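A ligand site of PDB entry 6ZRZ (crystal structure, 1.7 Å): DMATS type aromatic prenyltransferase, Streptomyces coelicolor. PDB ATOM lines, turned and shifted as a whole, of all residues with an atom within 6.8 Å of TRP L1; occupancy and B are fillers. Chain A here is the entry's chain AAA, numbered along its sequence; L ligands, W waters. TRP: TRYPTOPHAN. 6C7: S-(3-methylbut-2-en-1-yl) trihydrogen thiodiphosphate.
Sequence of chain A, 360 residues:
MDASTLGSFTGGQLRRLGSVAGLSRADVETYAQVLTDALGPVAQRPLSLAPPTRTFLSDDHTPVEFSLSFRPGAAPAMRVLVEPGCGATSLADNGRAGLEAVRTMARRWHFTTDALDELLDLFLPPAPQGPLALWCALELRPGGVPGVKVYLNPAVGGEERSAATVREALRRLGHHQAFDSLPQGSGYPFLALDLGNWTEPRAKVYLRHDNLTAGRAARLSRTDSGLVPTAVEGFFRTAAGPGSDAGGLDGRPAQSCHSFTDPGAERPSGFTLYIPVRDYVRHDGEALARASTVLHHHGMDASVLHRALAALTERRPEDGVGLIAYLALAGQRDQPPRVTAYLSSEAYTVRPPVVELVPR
NH2 of Arg 278 lies within salt-bridge range of OD1 of Asp 59. The backbone NH (N) of Leu 81 is in hydrogen-bond range of the backbone carbonyl oxygen (O) of Glu 65 (2.7 Å). The backbone carbonyl oxygen of Tyr 326 sits at hydrogen-bond distance from the backbone NH of Tyr 342, at 3.0 Å. The backbone NH (N) of Tyr 274 sits at hydrogen-bond distance from the backbone carbonyl oxygen (O) of Gln 255 (2.8 Å). N of Tyr 206 lies within hydrogen-bond range of O of Phe 190 (3.0 Å). NH1 of Arg 278 sits at hydrogen-bond distance from O of Ala 325, 2.9 Å away.
Phe 56 touches TRP L1 (CZ to OXT, 3.5 Å). Trp 135 touches TRP L1. Phe 190 touches TRP L1 (CE2 to CE3, 3.9 Å). Gln 255 touches TRP L1 (OE1 to CZ3, 3.7 Å). Tyr 274 touches TRP L1. Hydrophobic or aromatic side chains within 4 Å of TRP L1: Phe 56, Trp 135, Phe 190, Tyr 274 and Tyr 326.
Water W3 bridges OXT of TRP L1 and NE2 of Gln 255. Water W2 lies within hydrogen-bond range of the side-chain carboxylate of Asp 59 (2.6 Å), a nitrogen (N) of TRP L1 (2.7 Å) and the backbone carbonyl oxygen of Phe 56 (3.4 Å). Water W4 lies within hydrogen-bond range of OXT of TRP L1 (2.8 Å) and OH of Tyr 326 (3.5 Å). Water W5 lies within hydrogen-bond range of N of TRP L1 and OE2 of Glu 65. Water W1 bridges the guanidinium group (NH2) of Arg 252 and an oxygen (O) of TRP L1.
The side-chain hydroxyl (OH) of Tyr 342 sits at hydrogen-bond distance from an oxygen (O8) of 6C7 L2 (2.7 Å). S9 of 6C7 L2 lies close to OH of Tyr 206 (2.5 Å). O of Leu 57 lies within hydrogen-bond range of N of TRP L1 (2.9 Å). OH of Tyr 326 lies within hydrogen-bond range of O of TRP L1. The side-chain hydroxyl of Tyr 274 sits at hydrogen-bond distance from an oxygen (O8) of 6C7 L2 (2.6 Å). The guanidinium group of Arg 278 lies within salt-bridge range of an oxygen (O) of TRP L1, at 3.0 Å. The side-chain carboxylate (OE1) of Glu 65 is in hydrogen-bond range of a nitrogen (NE1) of TRP L1, at 2.8 Å.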
ATOM      1  N   PHE A  56      -8.823 -17.158  29.460  1.00  0.00           N
ATOM      2  CA  PHE A  56      -8.787 -16.306  28.225  1.00  0.00           C
ATOM      3  C   PHE A  56      -7.591 -16.673  27.319  1.00  0.00           C
ATOM      4  O   PHE A  56      -7.431 -16.102  26.199  1.00  0.00           O
ATOM      5  CB  PHE A  56      -8.679 -14.824  28.673  1.00  0.00           C
ATOM      6  CG  PHE A  56      -8.152 -13.781  27.688  1.00  0.00           C
ATOM      7  CD1 PHE A  56      -8.826 -13.474  26.516  1.00  0.00           C
ATOM      8  CD2 PHE A  56      -7.036 -13.026  28.004  1.00  0.00           C
ATOM      9  CE1 PHE A  56      -8.359 -12.486  25.666  1.00  0.00           C
ATOM     10  CE2 PHE A  56      -6.576 -12.035  27.160  1.00  0.00           C
ATOM     11  CZ  PHE A  56      -7.233 -11.770  25.990  1.00  0.00           C
ATOM     12  N   LEU A  57      -6.757 -17.600  27.761  1.00  0.00           N
ATOM     13  CA  LEU A  57      -5.441 -17.836  27.144  1.00  0.00           C
ATOM     14  C   LEU A  57      -5.616 -18.246  25.684  1.00  0.00           C
ATOM     15  O   LEU A  57      -4.761 -17.896  24.876  1.00  0.00           O
ATOM     16  CB  LEU A  57      -4.738 -18.922  27.934  1.00  0.00           C
ATOM     17  CG  LEU A  57      -3.291 -19.161  27.581  1.00  0.00           C
ATOM     18  CD1 LEU A  57      -2.529 -19.533  28.842  1.00  0.00           C
ATOM     19  CD2 LEU A  57      -3.166 -20.274  26.547  1.00  0.00           C
ATOM     20  N   SER A  58      -6.699 -18.930  25.370  1.00  0.00           N
ATOM     21  CA  SER A  58      -7.017 -19.414  24.013  1.00  0.00           C
ATOM     22  C   SER A  58      -8.504 -19.229  23.758  1.00  0.00           C
ATOM     23  O   SER A  58      -9.246 -19.138  24.711  1.00  0.00           O
ATOM     24  CB  SER A  58      -6.563 -20.835  23.845  1.00  0.00           C
ATOM     25  OG  SER A  58      -7.425 -21.744  24.540  1.00  0.00           O
ATOM     26  N   ASP A  59      -8.907 -19.230  22.493  1.00  0.00           N
ATOM     27  CA  ASP A  59     -10.312 -18.990  22.113  1.00  0.00           C
ATOM     28  C   ASP A  59     -11.221 -20.051  22.705  1.00  0.00           C
ATOM     29  O   ASP A  59     -12.336 -19.673  23.108  1.00  0.00           O
ATOM     30  CB  ASP A  59     -10.474 -18.954  20.602  1.00  0.00           C
ATOM     31  CG  ASP A  59     -10.031 -17.658  19.962  1.00  0.00           C
ATOM     32  OD1 ASP A  59      -9.389 -16.777  20.658  1.00  0.00           O
ATOM     33  OD2 ASP A  59     -10.318 -17.518  18.789  1.00  0.00           O
ATOM     34  N   GLU A  65      -1.201 -23.006  25.143  1.00  0.00           N
ATOM     35  CA  GLU A  65      -0.933 -22.689  23.723  1.00  0.00           C
ATOM     36  C   GLU A  65       0.517 -22.989  23.406  1.00  0.00           C
ATOM     37  O   GLU A  65       1.375 -22.845  24.302  1.00  0.00           O
ATOM     38  CB  GLU A  65      -1.269 -21.225  23.440  1.00  0.00           C
ATOM     39  CG  GLU A  65      -1.200 -20.881  21.983  1.00  0.00           C
ATOM     40  CD  GLU A  65      -1.443 -19.399  21.723  1.00  0.00           C
ATOM     41  OE1 GLU A  65      -0.506 -18.597  21.944  1.00  0.00           O
ATOM     42  OE2 GLU A  65      -2.536 -19.083  21.281  1.00  0.00           O
ATOM     43  N   LEU A  81       2.874 -21.963  26.419  1.00  0.00           N
ATOM     44  CA  LEU A  81       2.240 -20.928  27.256  1.00  0.00           C
ATOM     45  C   LEU A  81       1.171 -21.600  28.095  1.00  0.00           C
ATOM     46  O   LEU A  81       0.396 -22.391  27.545  1.00  0.00           O
ATOM     47  CB  LEU A  81       1.587 -19.887  26.350  1.00  0.00           C
ATOM     48  CG  LEU A  81       0.857 -18.762  27.065  1.00  0.00           C
ATOM     49  CD1 LEU A  81       1.846 -17.907  27.830  1.00  0.00           C
ATOM     50  CD2 LEU A  81       0.079 -17.933  26.074  1.00  0.00           C
ATOM     51  N   TRP A 135       0.323 -15.763  33.530  1.00  0.00           N
ATOM     52  CA  TRP A 135       0.662 -16.837  32.594  1.00  0.00           C
ATOM     53  C   TRP A 135       2.166 -17.040  32.656  1.00  0.00           C
ATOM     54  O   TRP A 135       2.905 -16.076  32.957  1.00  0.00           O
ATOM     55  CB  TRP A 135       0.196 -16.535  31.182  1.00  0.00           C
ATOM     56  CG  TRP A 135      -1.293 -16.376  31.041  1.00  0.00           C
ATOM     57  CD1 TRP A 135      -2.270 -16.781  31.895  1.00  0.00           C
ATOM     58  CD2 TRP A 135      -1.943 -15.791  29.912  1.00  0.00           C
ATOM     59  NE1 TRP A 135      -3.510 -16.479  31.363  1.00  0.00           N
ATOM     60  CE2 TRP A 135      -3.334 -15.880  30.145  1.00  0.00           C
ATOM     61  CE3 TRP A 135      -1.485 -15.228  28.720  1.00  0.00           C
ATOM     62  CZ2 TRP A 135      -4.267 -15.364  29.252  1.00  0.00           C
ATOM     63  CZ3 TRP A 135      -2.420 -14.704  27.838  1.00  0.00           C
ATOM     64  CH2 TRP A 135      -3.785 -14.802  28.104  1.00  0.00           C
ATOM     65  N   PRO A 189      -2.232  -4.909  27.053  1.00  0.00           N
ATOM     66  CA  PRO A 189      -2.778  -6.196  27.445  1.00  0.00           C
ATOM     67  C   PRO A 189      -1.861  -7.011  28.375  1.00  0.00           C
ATOM     68  O   PRO A 189      -2.394  -7.752  29.186  1.00  0.00           O
ATOM     69  CB  PRO A 189      -3.020  -6.968  26.137  1.00  0.00           C
ATOM     70  CG  PRO A 189      -2.324  -6.174  25.046  1.00  0.00           C
ATOM     71  CD  PRO A 189      -2.047  -4.788  25.593  1.00  0.00           C
ATOM     72  N   PHE A 190      -0.544  -6.868  28.243  1.00  0.00           N
ATOM     73  CA  PHE A 190       0.444  -7.681  28.989  1.00  0.00           C
ATOM     74  C   PHE A 190       1.669  -6.868  29.307  1.00  0.00           C
ATOM     75  O   PHE A 190       2.071  -5.987  28.489  1.00  0.00           O
ATOM     76  CB  PHE A 190       0.935  -8.891  28.192  1.00  0.00           C
ATOM     77  CG  PHE A 190      -0.165  -9.752  27.643  1.00  0.00           C
ATOM     78  CD1 PHE A 190      -0.887 -10.580  28.479  1.00  0.00           C
ATOM     79  CD2 PHE A 190      -0.458  -9.743  26.284  1.00  0.00           C
ATOM     80  CE1 PHE A 190      -1.913 -11.354  27.977  1.00  0.00           C
ATOM     81  CE2 PHE A 190      -1.473 -10.527  25.780  1.00  0.00           C
ATOM     82  CZ  PHE A 190      -2.222 -11.304  26.632  1.00  0.00           C
ATOM     83  N   TYR A 206       3.453  -4.994  25.984  1.00  0.00           N
ATOM     84  CA  TYR A 206       2.548  -5.285  24.857  1.00  0.00           C
ATOM     85  C   TYR A 206       1.522  -4.170  24.746  1.00  0.00           C
ATOM     86  O   TYR A 206       0.989  -3.701  25.816  1.00  0.00           O
ATOM     87  CB  TYR A 206       1.870  -6.638  25.052  1.00  0.00           C
ATOM     88  CG  TYR A 206       2.800  -7.809  25.005  1.00  0.00           C
ATOM     89  CD1 TYR A 206       2.857  -8.621  23.900  1.00  0.00           C
ATOM     90  CD2 TYR A 206       3.631  -8.119  26.079  1.00  0.00           C
ATOM     91  CE1 TYR A 206       3.695  -9.721  23.852  1.00  0.00           C
ATOM     92  CE2 TYR A 206       4.483  -9.216  26.030  1.00  0.00           C
ATOM     93  CZ  TYR A 206       4.529 -10.017  24.909  1.00  0.00           C
ATOM     94  OH  TYR A 206       5.351 -11.119  24.827  1.00  0.00           O
ATOM     95  N   ARG A 252     -10.194  -9.129  15.430  1.00  0.00           N
ATOM     96  CA  ARG A 252      -9.573  -8.837  16.709  1.00  0.00           C
ATOM     97  C   ARG A 252      -8.262  -8.120  16.390  1.00  0.00           C
ATOM     98  O   ARG A 252      -7.709  -8.241  15.303  1.00  0.00           O
ATOM     99  CB  ARG A 252      -9.486 -10.071  17.590  1.00  0.00           C
ATOM    100  CG  ARG A 252      -8.235 -10.847  17.381  1.00  0.00           C
ATOM    101  CD  ARG A 252      -8.224 -12.103  18.243  1.00  0.00           C
ATOM    102  NE  ARG A 252      -9.087 -13.148  17.679  1.00  0.00           N
ATOM    103  CZ  ARG A 252     -10.045 -13.866  18.317  1.00  0.00           C
ATOM    104  NH1 ARG A 252     -10.721 -14.782  17.638  1.00  0.00           N
ATOM    105  NH2 ARG A 252     -10.315 -13.692  19.608  1.00  0.00           N
ATOM    106  N   PRO A 253      -7.780  -7.306  17.325  1.00  0.00           N
ATOM    107  CA  PRO A 253      -6.687  -6.389  17.038  1.00  0.00           C
ATOM    108  C   PRO A 253      -5.307  -7.016  16.968  1.00  0.00           C
ATOM    109  O   PRO A 253      -5.019  -8.119  17.576  1.00  0.00           O
ATOM    110  CB  PRO A 253      -6.787  -5.434  18.176  1.00  0.00           C
ATOM    111  CG  PRO A 253      -7.241  -6.275  19.312  1.00  0.00           C
ATOM    112  CD  PRO A 253      -8.299  -7.175  18.683  1.00  0.00           C
ATOM    113  N   GLN A 255      -1.354  -6.751  17.936  1.00  0.00           N
ATOM    114  CA  GLN A 255      -0.648  -6.325  19.135  1.00  0.00           C
ATOM    115  C   GLN A 255       0.825  -6.129  18.764  1.00  0.00           C
ATOM    116  O   GLN A 255       1.267  -6.737  17.767  1.00  0.00           O
ATOM    117  CB  GLN A 255      -0.770  -7.384  20.237  1.00  0.00           C
ATOM    118  CG  GLN A 255      -2.181  -7.530  20.775  1.00  0.00           C
ATOM    119  CD  GLN A 255      -2.213  -8.305  22.072  1.00  0.00           C
ATOM    120  OE1 GLN A 255      -1.177  -8.526  22.750  1.00  0.00           O
ATOM    121  NE2 GLN A 255      -3.390  -8.745  22.421  1.00  0.00           N
ATOM    122  N   TYR A 274       2.345  -8.759  16.201  1.00  0.00           N
ATOM    123  CA  TYR A 274       1.464  -9.960  16.210  1.00  0.00           C
ATOM    124  C   TYR A 274       0.179  -9.702  15.435  1.00  0.00           C
ATOM    125  O   TYR A 274      -0.578  -8.745  15.760  1.00  0.00           O
ATOM    126  CB  TYR A 274       1.105 -10.347  17.637  1.00  0.00           C
ATOM    127  CG  TYR A 274       2.289 -10.523  18.568  1.00  0.00           C
ATOM    128  CD1 TYR A 274       2.773 -11.789  18.905  1.00  0.00           C
ATOM    129  CD2 TYR A 274       2.867  -9.415  19.172  1.00  0.00           C
ATOM    130  CE1 TYR A 274       3.877 -11.925  19.762  1.00  0.00           C
ATOM    131  CE2 TYR A 274       3.925  -9.539  20.050  1.00  0.00           C
ATOM    132  CZ  TYR A 274       4.439 -10.789  20.339  1.00  0.00           C
ATOM    133  OH  TYR A 274       5.514 -10.850  21.157  1.00  0.00           O
ATOM    134  N   PRO A 276      -3.433 -11.621  14.467  1.00  0.00           N
ATOM    135  CA  PRO A 276      -4.321 -12.771  14.733  1.00  0.00           C
ATOM    136  C   PRO A 276      -4.931 -13.331  13.450  1.00  0.00           C
ATOM    137  O   PRO A 276      -6.100 -13.161  13.178  1.00  0.00           O
ATOM    138  CB  PRO A 276      -5.374 -12.188  15.665  1.00  0.00           C
ATOM    139  CG  PRO A 276      -5.456 -10.745  15.231  1.00  0.00           C
ATOM    140  CD  PRO A 276      -4.062 -10.347  14.772  1.00  0.00           C
ATOM    141  N   ARG A 278      -6.080 -15.984  12.455  1.00  0.00           N
ATOM    142  CA  ARG A 278      -7.292 -16.822  12.535  1.00  0.00           C
ATOM    143  C   ARG A 278      -8.544 -16.010  12.201  1.00  0.00           C
ATOM    144  O   ARG A 278      -9.525 -16.630  11.768  1.00  0.00           O
ATOM    145  CB  ARG A 278      -7.483 -17.446  13.915  1.00  0.00           C
ATOM    146  CG  ARG A 278      -7.604 -16.463  15.068  1.00  0.00           C
ATOM    147  CD  ARG A 278      -7.468 -17.269  16.335  1.00  0.00           C
ATOM    148  NE  ARG A 278      -7.709 -16.567  17.602  1.00  0.00           N
ATOM    149  CZ  ARG A 278      -6.846 -15.782  18.255  1.00  0.00           C
ATOM    150  NH1 ARG A 278      -5.700 -15.459  17.716  1.00  0.00           N
ATOM    151  NH2 ARG A 278      -7.185 -15.254  19.426  1.00  0.00           N
ATOM    152  N   ALA A 325      -3.206 -19.440  15.493  1.00  0.00           N
ATOM    153  CA  ALA A 325      -3.899 -18.346  16.180  1.00  0.00           C
ATOM    154  C   ALA A 325      -3.305 -16.998  15.765  1.00  0.00           C
ATOM    155  O   ALA A 325      -4.083 -16.062  15.447  1.00  0.00           O
ATOM    156  CB  ALA A 325      -3.832 -18.538  17.643  1.00  0.00           C
ATOM    157  N   TYR A 326      -1.991 -16.862  15.835  1.00  0.00           N
ATOM    158  CA  TYR A 326      -1.261 -15.628  15.486  1.00  0.00           C
ATOM    159  C   TYR A 326      -0.049 -15.987  14.642  1.00  0.00           C
ATOM    160  O   TYR A 326       0.530 -17.066  14.769  1.00  0.00           O
ATOM    161  CB  TYR A 326      -0.693 -14.892  16.701  1.00  0.00           C
ATOM    162  CG  TYR A 326      -1.662 -14.116  17.534  1.00  0.00           C
ATOM    163  CD1 TYR A 326      -1.877 -12.768  17.300  1.00  0.00           C
ATOM    164  CD2 TYR A 326      -2.394 -14.734  18.516  1.00  0.00           C
ATOM    165  CE1 TYR A 326      -2.752 -12.023  18.096  1.00  0.00           C
ATOM    166  CE2 TYR A 326      -3.304 -14.030  19.283  1.00  0.00           C
ATOM    167  CZ  TYR A 326      -3.494 -12.660  19.072  1.00  0.00           C
ATOM    168  OH  TYR A 326      -4.407 -11.948  19.834  1.00  0.00           O
ATOM    169  N   TYR A 342       1.928 -19.132  16.465  1.00  0.00           N
ATOM    170  CA  TYR A 342       1.218 -19.501  17.697  1.00  0.00           C
ATOM    171  C   TYR A 342       0.176 -20.525  17.326  1.00  0.00           C
ATOM    172  O   TYR A 342      -0.657 -20.250  16.447  1.00  0.00           O
ATOM    173  CB  TYR A 342       0.673 -18.226  18.351  1.00  0.00           C
ATOM    174  CG  TYR A 342       1.796 -17.337  18.761  1.00  0.00           C
ATOM    175  CD1 TYR A 342       2.329 -17.388  20.038  1.00  0.00           C
ATOM    176  CD2 TYR A 342       2.427 -16.523  17.808  1.00  0.00           C
ATOM    177  CE1 TYR A 342       3.452 -16.628  20.376  1.00  0.00           C
ATOM    178  CE2 TYR A 342       3.487 -15.716  18.154  1.00  0.00           C
ATOM    179  CZ  TYR A 342       4.026 -15.791  19.429  1.00  0.00           C
ATOM    180  OH  TYR A 342       5.110 -15.026  19.736  1.00  0.00           O
HETATM  181  N   TRP L   1      -5.608 -15.699  23.191  1.00  0.00           N
HETATM  182  CA  TRP L   1      -5.328 -14.351  23.752  1.00  0.00           C
HETATM  183  C   TRP L   1      -5.466 -13.279  22.657  1.00  0.00           C
HETATM  184  O   TRP L   1      -5.670 -13.551  21.450  1.00  0.00           O
HETATM  185  CB  TRP L   1      -3.947 -14.301  24.410  1.00  0.00           C
HETATM  186  CG  TRP L   1      -2.798 -14.730  23.544  1.00  0.00           C
HETATM  187  CD1 TRP L   1      -2.308 -16.001  23.405  1.00  0.00           C
HETATM  188  CD2 TRP L   1      -1.990 -13.896  22.715  1.00  0.00           C
HETATM  189  NE1 TRP L   1      -1.256 -16.006  22.523  1.00  0.00           N
HETATM  190  CE2 TRP L   1      -1.019 -14.718  22.099  1.00  0.00           C
HETATM  191  CE3 TRP L   1      -1.966 -12.518  22.437  1.00  0.00           C
HETATM  192  CZ2 TRP L   1      -0.059 -14.227  21.216  1.00  0.00           C
HETATM  193  CZ3 TRP L   1      -1.018 -12.031  21.573  1.00  0.00           C
HETATM  194  CH2 TRP L   1      -0.089 -12.864  20.959  1.00  0.00           C
HETATM  195  OXT TRP L   1      -5.388 -12.072  22.993  1.00  0.00           O
HETATM  196  O4  6C7 L   2      10.002 -12.511  22.258  1.00  0.00           O
HETATM  197  P1  6C7 L   2       9.290 -13.914  22.678  1.00  0.00           P
HETATM  198  O6  6C7 L   2       9.256 -14.907  21.581  1.00  0.00           O
HETATM  199  O5  6C7 L   2      10.150 -14.461  23.963  1.00  0.00           O
HETATM  200  O2  6C7 L   2       7.831 -13.573  23.317  1.00  0.00           O
HETATM  201  P3  6C7 L   2       6.445 -14.063  22.640  1.00  0.00           P
HETATM  202  O8  6C7 L   2       6.434 -13.257  21.237  1.00  0.00           O
HETATM  203  O7  6C7 L   2       6.319 -15.517  22.398  1.00  0.00           O
HETATM  204  S9  6C7 L   2       5.120 -13.346  23.638  1.00  0.00           S
HETATM  205  C10 6C7 L   2       3.661 -13.857  22.710  1.00  0.00           C
HETATM  206  C11 6C7 L   2       2.740 -14.521  23.783  1.00  0.00           C
HETATM  207  C12 6C7 L   2       1.639 -13.733  24.521  1.00  0.00           C
HETATM  208  C13 6C7 L   2       0.799 -14.433  25.558  1.00  0.00           C
HETATM  209  C14 6C7 L   2       1.365 -12.250  24.258  1.00  0.00           C
HETATM  210  O   HOH W   1      -8.757 -12.714  21.657  1.00  0.00           O
HETATM  211  O   HOH W   2      -8.327 -15.962  22.911  1.00  0.00           O
HETATM  212  O   HOH W   3      -4.677 -10.039  24.405  1.00  0.00           O
HETATM  213  O   HOH W   4      -7.071 -10.442  21.528  1.00  0.00           O
HETATM  214  O   HOH W   5      -4.397 -16.898  20.839  1.00  0.00           O
